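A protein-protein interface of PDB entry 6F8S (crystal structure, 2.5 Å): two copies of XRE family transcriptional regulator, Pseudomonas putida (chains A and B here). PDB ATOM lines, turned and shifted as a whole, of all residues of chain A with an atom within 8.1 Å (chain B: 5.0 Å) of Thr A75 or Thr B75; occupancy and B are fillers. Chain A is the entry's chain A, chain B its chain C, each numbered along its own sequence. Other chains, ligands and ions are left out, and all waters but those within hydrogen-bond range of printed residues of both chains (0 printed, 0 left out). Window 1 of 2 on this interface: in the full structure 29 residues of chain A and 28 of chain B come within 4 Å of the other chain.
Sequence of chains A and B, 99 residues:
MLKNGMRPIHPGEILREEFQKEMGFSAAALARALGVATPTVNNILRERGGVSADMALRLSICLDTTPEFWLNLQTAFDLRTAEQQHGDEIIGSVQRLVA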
ATOM      1  N   ILE A   9      11.411  22.463 -10.305  1.00  0.00           N
ATOM      2  CA  ILE A   9      10.190  21.998 -10.951  1.00  0.00           C
ATOM      3  C   ILE A   9       8.994  22.237 -10.042  1.00  0.00           C
ATOM      4  O   ILE A   9       8.812  21.585  -9.019  1.00  0.00           O
ATOM      5  CB  ILE A   9      10.312  20.518 -11.355  1.00  0.00           C
ATOM      6  CG1 ILE A   9      11.434  20.411 -12.420  1.00  0.00           C
ATOM      7  CG2 ILE A   9       8.983  20.001 -11.879  1.00  0.00           C
ATOM      8  CD1 ILE A   9      11.634  19.040 -13.037  1.00  0.00           C
ATOM      9  N   PRO A  11       5.418  22.246  -8.466  1.00  0.00           N
ATOM     10  CA  PRO A  11       4.355  21.228  -8.420  1.00  0.00           C
ATOM     11  C   PRO A  11       3.226  21.546  -9.400  1.00  0.00           C
ATOM     12  O   PRO A  11       2.537  20.635  -9.875  1.00  0.00           O
ATOM     13  CB  PRO A  11       3.868  21.275  -6.960  1.00  0.00           C
ATOM     14  CG  PRO A  11       4.523  22.494  -6.345  1.00  0.00           C
ATOM     15  CD  PRO A  11       5.782  22.727  -7.120  1.00  0.00           C
ATOM     16  N   VAL A  51       1.972  24.956  -2.839  1.00  0.00           N
ATOM     17  CA  VAL A  51       0.970  24.020  -2.364  1.00  0.00           C
ATOM     18  C   VAL A  51       1.104  23.851  -0.855  1.00  0.00           C
ATOM     19  O   VAL A  51       2.147  23.398  -0.367  1.00  0.00           O
ATOM     20  CB  VAL A  51       1.104  22.631  -3.052  1.00  0.00           C
ATOM     21  CG1 VAL A  51      -0.032  21.706  -2.606  1.00  0.00           C
ATOM     22  CG2 VAL A  51       1.091  22.777  -4.557  1.00  0.00           C
ATOM     23  N   ALA A  53      -0.066  22.238   2.924  1.00  0.00           N
ATOM     24  CA  ALA A  53      -0.373  20.898   3.419  1.00  0.00           C
ATOM     25  C   ALA A  53      -1.850  20.562   3.178  1.00  0.00           C
ATOM     26  O   ALA A  53      -2.196  19.426   2.807  1.00  0.00           O
ATOM     27  CB  ALA A  53      -0.027  20.789   4.909  1.00  0.00           C
ATOM     28  N   PRO A  67      -0.397  12.830  -0.168  1.00  0.00           N
ATOM     29  CA  PRO A  67      -0.196  14.273   0.014  1.00  0.00           C
ATOM     30  C   PRO A  67       1.291  14.630   0.072  1.00  0.00           C
ATOM     31  O   PRO A  67       1.655  15.756  -0.264  1.00  0.00           O
ATOM     32  CB  PRO A  67      -0.899  14.560   1.357  1.00  0.00           C
ATOM     33  CG  PRO A  67      -0.828  13.274   2.062  1.00  0.00           C
ATOM     34  CD  PRO A  67      -0.998  12.208   1.026  1.00  0.00           C
ATOM     35  N   GLU A  68       2.130  13.682   0.484  1.00  0.00           N
ATOM     36  CA  GLU A  68       3.568  13.893   0.550  1.00  0.00           C
ATOM     37  C   GLU A  68       4.171  14.042  -0.842  1.00  0.00           C
ATOM     38  O   GLU A  68       5.197  14.726  -1.021  1.00  0.00           O
ATOM     39  CB  GLU A  68       4.251  12.739   1.285  1.00  0.00           C
ATOM     40  CG  GLU A  68       4.014  12.761   2.761  1.00  0.00           C
ATOM     41  CD  GLU A  68       2.955  11.767   3.216  1.00  0.00           C
ATOM     42  OE1 GLU A  68       2.085  11.382   2.383  1.00  0.00           O
ATOM     43  OE2 GLU A  68       2.999  11.386   4.422  1.00  0.00           O
ATOM     44  N   PHE A  69       3.560  13.376  -1.819  1.00  0.00           N
ATOM     45  CA  PHE A  69       3.957  13.562  -3.208  1.00  0.00           C
ATOM     46  C   PHE A  69       3.993  15.055  -3.546  1.00  0.00           C
ATOM     47  O   PHE A  69       4.992  15.571  -4.071  1.00  0.00           O
ATOM     48  CB  PHE A  69       2.994  12.818  -4.139  1.00  0.00           C
ATOM     49  CG  PHE A  69       3.297  12.995  -5.611  1.00  0.00           C
ATOM     50  CD1 PHE A  69       4.426  12.418  -6.169  1.00  0.00           C
ATOM     51  CD2 PHE A  69       2.424  13.706  -6.430  1.00  0.00           C
ATOM     52  CE1 PHE A  69       4.705  12.568  -7.516  1.00  0.00           C
ATOM     53  CE2 PHE A  69       2.682  13.860  -7.768  1.00  0.00           C
ATOM     54  CZ  PHE A  69       3.832  13.286  -8.325  1.00  0.00           C
ATOM     55  N   TRP A  70       2.911  15.755  -3.218  1.00  0.00           N
ATOM     56  CA  TRP A  70       2.828  17.161  -3.570  1.00  0.00           C
ATOM     57  C   TRP A  70       3.750  18.037  -2.706  1.00  0.00           C
ATOM     58  O   TRP A  70       4.348  18.992  -3.201  1.00  0.00           O
ATOM     59  CB  TRP A  70       1.371  17.630  -3.487  1.00  0.00           C
ATOM     60  CG  TRP A  70       0.512  16.897  -4.489  1.00  0.00           C
ATOM     61  CD1 TRP A  70      -0.322  15.841  -4.242  1.00  0.00           C
ATOM     62  CD2 TRP A  70       0.443  17.136  -5.905  1.00  0.00           C
ATOM     63  NE1 TRP A  70      -0.908  15.418  -5.411  1.00  0.00           N
ATOM     64  CE2 TRP A  70      -0.458  16.197  -6.443  1.00  0.00           C
ATOM     65  CE3 TRP A  70       1.054  18.048  -6.758  1.00  0.00           C
ATOM     66  CZ2 TRP A  70      -0.772  16.153  -7.807  1.00  0.00           C
ATOM     67  CZ3 TRP A  70       0.743  17.998  -8.124  1.00  0.00           C
ATOM     68  CH2 TRP A  70      -0.165  17.059  -8.628  1.00  0.00           C
ATOM     69  N   LEU A  71       3.896  17.703  -1.429  1.00  0.00           N
ATOM     70  CA  LEU A  71       4.736  18.509  -0.547  1.00  0.00           C
ATOM     71  C   LEU A  71       6.220  18.302  -0.869  1.00  0.00           C
ATOM     72  O   LEU A  71       7.022  19.247  -0.774  1.00  0.00           O
ATOM     73  CB  LEU A  71       4.437  18.180   0.933  1.00  0.00           C
ATOM     74  CG  LEU A  71       3.057  18.675   1.362  1.00  0.00           C
ATOM     75  CD1 LEU A  71       2.739  18.259   2.773  1.00  0.00           C
ATOM     76  CD2 LEU A  71       3.049  20.182   1.232  1.00  0.00           C
ATOM     77  N   ASN A  72       6.583  17.081  -1.262  1.00  0.00           N
ATOM     78  CA  ASN A  72       7.957  16.801  -1.688  1.00  0.00           C
ATOM     79  C   ASN A  72       8.382  17.599  -2.917  1.00  0.00           C
ATOM     80  O   ASN A  72       9.549  18.014  -3.032  1.00  0.00           O
ATOM     81  CB  ASN A  72       8.149  15.311  -1.984  1.00  0.00           C
ATOM     82  CG  ASN A  72       8.123  14.465  -0.724  1.00  0.00           C
ATOM     83  OD1 ASN A  72       8.199  14.994   0.393  1.00  0.00           O
ATOM     84  ND2 ASN A  72       8.017  13.157  -0.890  1.00  0.00           N
ATOM     85  N   LEU A  73       7.440  17.803  -3.840  1.00  0.00           N
ATOM     86  CA  LEU A  73       7.721  18.574  -5.046  1.00  0.00           C
ATOM     87  C   LEU A  73       7.894  20.046  -4.658  1.00  0.00           C
ATOM     88  O   LEU A  73       8.803  20.736  -5.152  1.00  0.00           O
ATOM     89  CB  LEU A  73       6.605  18.393  -6.080  1.00  0.00           C
ATOM     90  CG  LEU A  73       6.447  16.985  -6.677  1.00  0.00           C
ATOM     91  CD1 LEU A  73       5.056  16.829  -7.320  1.00  0.00           C
ATOM     92  CD2 LEU A  73       7.540  16.631  -7.679  1.00  0.00           C
ATOM     93  N   GLN A  74       7.042  20.500  -3.741  1.00  0.00           N
ATOM     94  CA  GLN A  74       7.094  21.862  -3.231  1.00  0.00           C
ATOM     95  C   GLN A  74       8.394  22.096  -2.474  1.00  0.00           C
ATOM     96  O   GLN A  74       9.040  23.142  -2.604  1.00  0.00           O
ATOM     97  CB  GLN A  74       5.906  22.137  -2.316  1.00  0.00           C
ATOM     98  CG  GLN A  74       5.858  23.569  -1.848  1.00  0.00           C
ATOM     99  CD  GLN A  74       5.560  24.500  -2.987  1.00  0.00           C
ATOM    100  OE1 GLN A  74       4.594  24.301  -3.721  1.00  0.00           O
ATOM    101  NE2 GLN A  74       6.402  25.506  -3.168  1.00  0.00           N
ATOM    102  N   THR A  75       8.782  21.096  -1.691  1.00  0.00           N
ATOM    103  CA  THR A  75      10.023  21.162  -0.930  1.00  0.00           C
ATOM    104  C   THR A  75      11.248  21.233  -1.847  1.00  0.00           C
ATOM    105  O   THR A  75      12.147  22.057  -1.633  1.00  0.00           O
ATOM    106  CB  THR A  75      10.114  19.965   0.014  1.00  0.00           C
ATOM    107  OG1 THR A  75       9.397  20.284   1.215  1.00  0.00           O
ATOM    108  CG2 THR A  75      11.559  19.637   0.365  1.00  0.00           C
ATOM    109  N   ALA A  76      11.269  20.381  -2.874  1.00  0.00           N
ATOM    110  CA  ALA A  76      12.405  20.322  -3.783  1.00  0.00           C
ATOM    111  C   ALA A  76      12.458  21.626  -4.561  1.00  0.00           C
ATOM    112  O   ALA A  76      13.531  22.171  -4.777  1.00  0.00           O
ATOM    113  CB  ALA A  76      12.313  19.107  -4.731  1.00  0.00           C
ATOM    114  N   PHE A  77      11.285  22.148  -4.920  1.00  0.00           N
ATOM    115  CA  PHE A  77      11.204  23.398  -5.657  1.00  0.00           C
ATOM    116  C   PHE A  77      11.685  24.608  -4.864  1.00  0.00           C
ATOM    117  O   PHE A  77      12.492  25.396  -5.362  1.00  0.00           O
ATOM    118  CB  PHE A  77       9.775  23.661  -6.123  1.00  0.00           C
ATOM    119  CG  PHE A  77       9.620  24.979  -6.839  1.00  0.00           C
ATOM    120  CD1 PHE A  77      10.006  25.107  -8.168  1.00  0.00           C
ATOM    121  CD2 PHE A  77       9.101  26.087  -6.189  1.00  0.00           C
ATOM    122  CE1 PHE A  77       9.876  26.312  -8.834  1.00  0.00           C
ATOM    123  CE2 PHE A  77       8.977  27.302  -6.854  1.00  0.00           C
ATOM    124  CZ  PHE A  77       9.364  27.411  -8.173  1.00  0.00           C
ATOM    125  N   ASP A  78      11.157  24.783  -3.654  1.00  0.00           N
ATOM    126  CA  ASP A  78      11.567  25.904  -2.825  1.00  0.00           C
ATOM    127  C   ASP A  78      13.063  25.845  -2.571  1.00  0.00           C
ATOM    128  O   ASP A  78      13.739  26.877  -2.543  1.00  0.00           O
ATOM    129  CB  ASP A  78      10.810  25.914  -1.486  1.00  0.00           C
ATOM    130  CG  ASP A  78       9.333  26.265  -1.646  1.00  0.00           C
ATOM    131  OD1 ASP A  78       9.009  27.067  -2.559  1.00  0.00           O
ATOM    132  OD2 ASP A  78       8.503  25.727  -0.866  1.00  0.00           O
ATOM    133  N   LEU A  79      13.573  24.631  -2.385  1.00  0.00           N
ATOM    134  CA  LEU A  79      14.970  24.460  -2.028  1.00  0.00           C
ATOM    135  C   LEU A  79      15.901  24.732  -3.212  1.00  0.00           C
ATOM    136  O   LEU A  79      16.913  25.409  -3.035  1.00  0.00           O
ATOM    137  CB  LEU A  79      15.214  23.061  -1.462  1.00  0.00           C
ATOM    138  CG  LEU A  79      16.617  22.748  -0.922  1.00  0.00           C
ATOM    139  CD1 LEU A  79      17.143  23.884  -0.058  1.00  0.00           C
ATOM    140  CD2 LEU A  79      16.596  21.438  -0.130  1.00  0.00           C
ATOM    141  N   ARG A  80      15.570  24.232  -4.405  1.00  0.00           N
ATOM    142  CA  ARG A  80      16.407  24.528  -5.578  1.00  0.00           C
ATOM    143  C   ARG A  80      16.404  26.019  -5.844  1.00  0.00           C
ATOM    144  O   ARG A  80      17.451  26.617  -6.133  1.00  0.00           O
ATOM    145  CB  ARG A  80      15.928  23.788  -6.829  1.00  0.00           C
ATOM    146  CG  ARG A  80      16.227  22.305  -6.815  1.00  0.00           C
ATOM    147  CD  ARG A  80      17.720  22.032  -6.838  1.00  0.00           C
ATOM    148  NE  ARG A  80      18.301  22.725  -7.964  1.00  0.00           N
ATOM    149  CZ  ARG A  80      19.381  23.486  -7.891  1.00  0.00           C
ATOM    150  NH1 ARG A  80      20.036  23.633  -6.738  1.00  0.00           N
ATOM    151  NH2 ARG A  80      19.816  24.083  -8.988  1.00  0.00           N
ATOM    152  N   THR A  81      15.219  26.619  -5.752  1.00  0.00           N
ATOM    153  CA  THR A  81      15.089  28.058  -5.955  1.00  0.00           C
ATOM    154  C   THR A  81      16.019  28.812  -5.009  1.00  0.00           C
ATOM    155  O   THR A  81      16.918  29.503  -5.452  1.00  0.00           O
ATOM    156  CB  THR A  81      13.651  28.528  -5.739  1.00  0.00           C
ATOM    157  OG1 THR A  81      12.806  27.883  -6.697  1.00  0.00           O
ATOM    158  CG2 THR A  81      13.561  30.036  -5.912  1.00  0.00           C
ATOM    159  N   ALA A  82      15.816  28.629  -3.706  1.00  0.00           N
ATOM    160  CA  ALA A  82      16.649  29.241  -2.666  1.00  0.00           C
ATOM    161  C   ALA A  82      18.140  29.053  -2.944  1.00  0.00           C
ATOM    162  O   ALA A  82      18.916  30.010  -2.917  1.00  0.00           O
ATOM    163  CB  ALA A  82      16.283  28.656  -1.289  1.00  0.00           C
ATOM    164  N   LEU B  71      13.238  20.616   6.072  1.00  0.00           N
ATOM    165  CA  LEU B  71      11.987  20.755   5.334  1.00  0.00           C
ATOM    166  C   LEU B  71      11.105  19.510   5.444  1.00  0.00           C
ATOM    167  O   LEU B  71       9.868  19.615   5.434  1.00  0.00           O
ATOM    168  CB  LEU B  71      12.262  21.065   3.858  1.00  0.00           C
ATOM    169  CG  LEU B  71      12.872  22.439   3.617  1.00  0.00           C
ATOM    170  CD1 LEU B  71      13.170  22.611   2.161  1.00  0.00           C
ATOM    171  CD2 LEU B  71      11.883  23.482   4.086  1.00  0.00           C
ATOM    172  N   ASN B  72      11.732  18.342   5.553  1.00  0.00           N
ATOM    173  CA  ASN B  72      10.993  17.105   5.806  1.00  0.00           C
ATOM    174  C   ASN B  72      10.247  17.123   7.131  1.00  0.00           C
ATOM    175  O   ASN B  72       9.112  16.635   7.221  1.00  0.00           O
ATOM    176  CB  ASN B  72      11.930  15.896   5.766  1.00  0.00           C
ATOM    177  CG  ASN B  72      12.393  15.594   4.359  1.00  0.00           C
ATOM    178  OD1 ASN B  72      11.810  16.101   3.400  1.00  0.00           O
ATOM    179  ND2 ASN B  72      13.446  14.801   4.220  1.00  0.00           N
ATOM    180  N   LEU B  73      10.876  17.685   8.161  1.00  0.00           N
ATOM    181  CA  LEU B  73      10.224  17.769   9.457  1.00  0.00           C
ATOM    182  C   LEU B  73       9.080  18.783   9.338  1.00  0.00           C
ATOM    183  O   LEU B  73       7.993  18.588   9.912  1.00  0.00           O
ATOM    184  CB  LEU B  73      11.220  18.164  10.558  1.00  0.00           C
ATOM    185  CG  LEU B  73      12.341  17.186  10.949  1.00  0.00           C
ATOM    186  CD1 LEU B  73      13.380  17.923  11.776  1.00  0.00           C
ATOM    187  CD2 LEU B  73      11.861  15.958  11.707  1.00  0.00           C
ATOM    188  N   GLN B  74       9.305  19.836   8.550  1.00  0.00           N
ATOM    189  CA  GLN B  74       8.279  20.863   8.372  1.00  0.00           C
ATOM    190  C   GLN B  74       7.120  20.285   7.587  1.00  0.00           C
ATOM    191  O   GLN B  74       5.953  20.538   7.880  1.00  0.00           O
ATOM    192  CB  GLN B  74       8.835  22.089   7.660  1.00  0.00           C
ATOM    193  CG  GLN B  74       7.841  23.236   7.585  1.00  0.00           C
ATOM    194  CD  GLN B  74       7.573  23.862   8.943  1.00  0.00           C
ATOM    195  OE1 GLN B  74       8.503  24.203   9.685  1.00  0.00           O
ATOM    196  NE2 GLN B  74       6.298  24.001   9.285  1.00  0.00           N
ATOM    197  N   THR B  75       7.458  19.475   6.598  1.00  0.00           N
ATOM    198  CA  THR B  75       6.457  18.788   5.801  1.00  0.00           C
ATOM    199  C   THR B  75       5.551  17.894   6.646  1.00  0.00           C
ATOM    200  O   THR B  75       4.314  17.997   6.577  1.00  0.00           O
ATOM    201  CB  THR B  75       7.145  17.977   4.721  1.00  0.00           C
ATOM    202  OG1 THR B  75       7.456  18.866   3.646  1.00  0.00           O
ATOM    203  CG2 THR B  75       6.247  16.856   4.193  1.00  0.00           C
ATOM    204  N   ALA B  76       6.177  17.037   7.456  1.00  0.00           N
ATOM    205  CA  ALA B  76       5.450  16.043   8.214  1.00  0.00           C
ATOM    206  C   ALA B  76       4.604  16.754   9.273  1.00  0.00           C
ATOM    207  O   ALA B  76       3.482  16.332   9.564  1.00  0.00           O
ATOM    208  CB  ALA B  76       6.424  15.021   8.851  1.00  0.00           C
ATOM    209  N   PHE B  77       5.128  17.859   9.808  1.00  0.00           N
ATOM    210  CA  PHE B  77       4.390  18.605  10.818  1.00  0.00           C
ATOM    211  C   PHE B  77       3.181  19.299  10.231  1.00  0.00           C
ATOM    212  O   PHE B  77       2.104  19.217  10.789  1.00  0.00           O
ATOM    213  CB  PHE B  77       5.274  19.640  11.506  1.00  0.00           C
ATOM    214  CG  PHE B  77       4.513  20.554  12.448  1.00  0.00           C
ATOM    215  CD1 PHE B  77       4.167  20.123  13.729  1.00  0.00           C
ATOM    216  CD2 PHE B  77       4.162  21.849  12.060  1.00  0.00           C
ATOM    217  CE1 PHE B  77       3.476  20.954  14.599  1.00  0.00           C
ATOM    218  CE2 PHE B  77       3.476  22.681  12.919  1.00  0.00           C
ATOM    219  CZ  PHE B  77       3.125  22.236  14.191  1.00  0.00           C
ATOM    220  N   ASP B  78       3.368  20.004   9.121  1.00  0.00           N
ATOM    221  CA  ASP B  78       2.253  20.661   8.458  1.00  0.00           C
ATOM    222  C   ASP B  78       1.215  19.644   8.050  1.00  0.00           C
ATOM    223  O   ASP B  78       0.019  19.913   8.103  1.00  0.00           O
ATOM    224  CB  ASP B  78       2.718  21.440   7.220  1.00  0.00           C
ATOM    225  CG  ASP B  78       3.470  22.710   7.570  1.00  0.00           C
ATOM    226  OD1 ASP B  78       3.251  23.223   8.693  1.00  0.00           O
ATOM    227  OD2 ASP B  78       4.284  23.183   6.729  1.00  0.00           O
ATOM    228  N   LEU B  79       1.672  18.474   7.625  1.00  0.00           N
ATOM    229  CA  LEU B  79       0.736  17.466   7.158  1.00  0.00           C
ATOM    230  C   LEU B  79       0.017  16.761   8.317  1.00  0.00           C
ATOM    231  O   LEU B  79      -1.202  16.593   8.238  1.00  0.00           O
ATOM    232  CB  LEU B  79       1.438  16.450   6.252  1.00  0.00           C
ATOM    233  CG  LEU B  79       0.576  15.342   5.623  1.00  0.00           C
ATOM    234  CD1 LEU B  79      -0.697  15.908   4.999  1.00  0.00           C
ATOM    235  CD2 LEU B  79       1.397  14.602   4.577  1.00  0.00           C
ATOM    236  N   ARG B  80       0.721  16.367   9.385  1.00  0.00           N
ATOM    237  CA  ARG B  80      -0.005  15.782  10.539  1.00  0.00           C
ATOM    238  C   ARG B  80      -1.026  16.774  11.050  1.00  0.00           C
ATOM    239  O   ARG B  80      -2.158  16.409  11.358  1.00  0.00           O
ATOM    240  CB  ARG B  80       0.911  15.383  11.710  1.00  0.00           C
ATOM    241  CG  ARG B  80       1.694  14.087  11.548  1.00  0.00           C
ATOM    242  CD  ARG B  80       0.806  12.871  11.299  1.00  0.00           C
ATOM    243  NE  ARG B  80      -0.164  12.709  12.362  1.00  0.00           N
ATOM    244  CZ  ARG B  80      -1.463  12.524  12.169  1.00  0.00           C
ATOM    245  NH1 ARG B  80      -1.964  12.463  10.939  1.00  0.00           N
ATOM    246  NH2 ARG B  80      -2.264  12.394  13.213  1.00  0.00           N
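The side-chain hydroxyl (OG1) of Thr B75 lies within hydrogen-bond range of the side-chain hydroxyl (OG1) of Thr A75, 3.4 Å away.
ND2 of Asn A72 sits close to O of Glu A68.
The backbone carbonyl oxygen (O) of Leu A71 lies within hydrogen-bond range of the side-chain hydroxyl (OG1) of Thr A75.
The backbone carbonyl oxygen (O) of Leu B71 is in hydrogen-bond range of the side-chain hydroxyl (OG1) of Thr B75 (3.1 Å).
OD1 of Asp B78 lies within hydrogen-bond range of NE2 of Gln B74, 3.2 Å away.
O of Asp B78 touches CB of Ala A53, 3.3 Å away.
Leu B79 touches Ala A53.
Leu B79 touches Pro A67.
Glu A68 touches Leu B79 (CD to CD2, 3.5 Å).
CG2 of Thr B75 touches CB of Leu A71, 3.96 Å away.
Thr A75 touches Leu B71.
Of chain B, only Leu B71 (3.8 Å) and Thr B75 (3.4 Å) come within 4 Å of Thr A75.
Of chain A, only Leu A71 (3.96 Å) and Thr A75 (3.4 Å) come within 4 Å of Thr B75.
No residue of chain A comes within 4 Å of Ala B76.
Of the printed residues of chain A, Leu B79 touches Ala A53 (3.95 Å), Pro A67 (3.6 Å) and Glu A68 (3.5 Å).
Of the printed residues of chain B, Glu A68 touches Leu B79 (3.5 Å).
Of the printed residues of chain A, Asp B78 touches Ala A53 (3.3 Å).
Leu A73 touches none of the printed residues of chain B.
The nearest printed residue of chain A that does not touch Leu B71 is Leu A79 (4.2 Å).
Printed residues of chain B that touch a printed residue of chain A: Leu B71, Thr B75, Asp B78 and Leu B79.
Hydrophobic or aromatic side chains of chain B that line the printed part of chain A: Leu B71 and Leu B79.
Among the printed residues, no Asp or Glu carboxylate lies within 4 Å of a Lys or Arg side-chain nitrogen of the other chain.
Leu A71 touches Thr B75, and with the chains exchanged Thr A75 touches Leu B71.
Thr A75 touches its own counterpart, Thr B75.
Of the 7 pairs that touch across the chains among the printed residues, 3 have their exchanged pair printed and touching as well.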
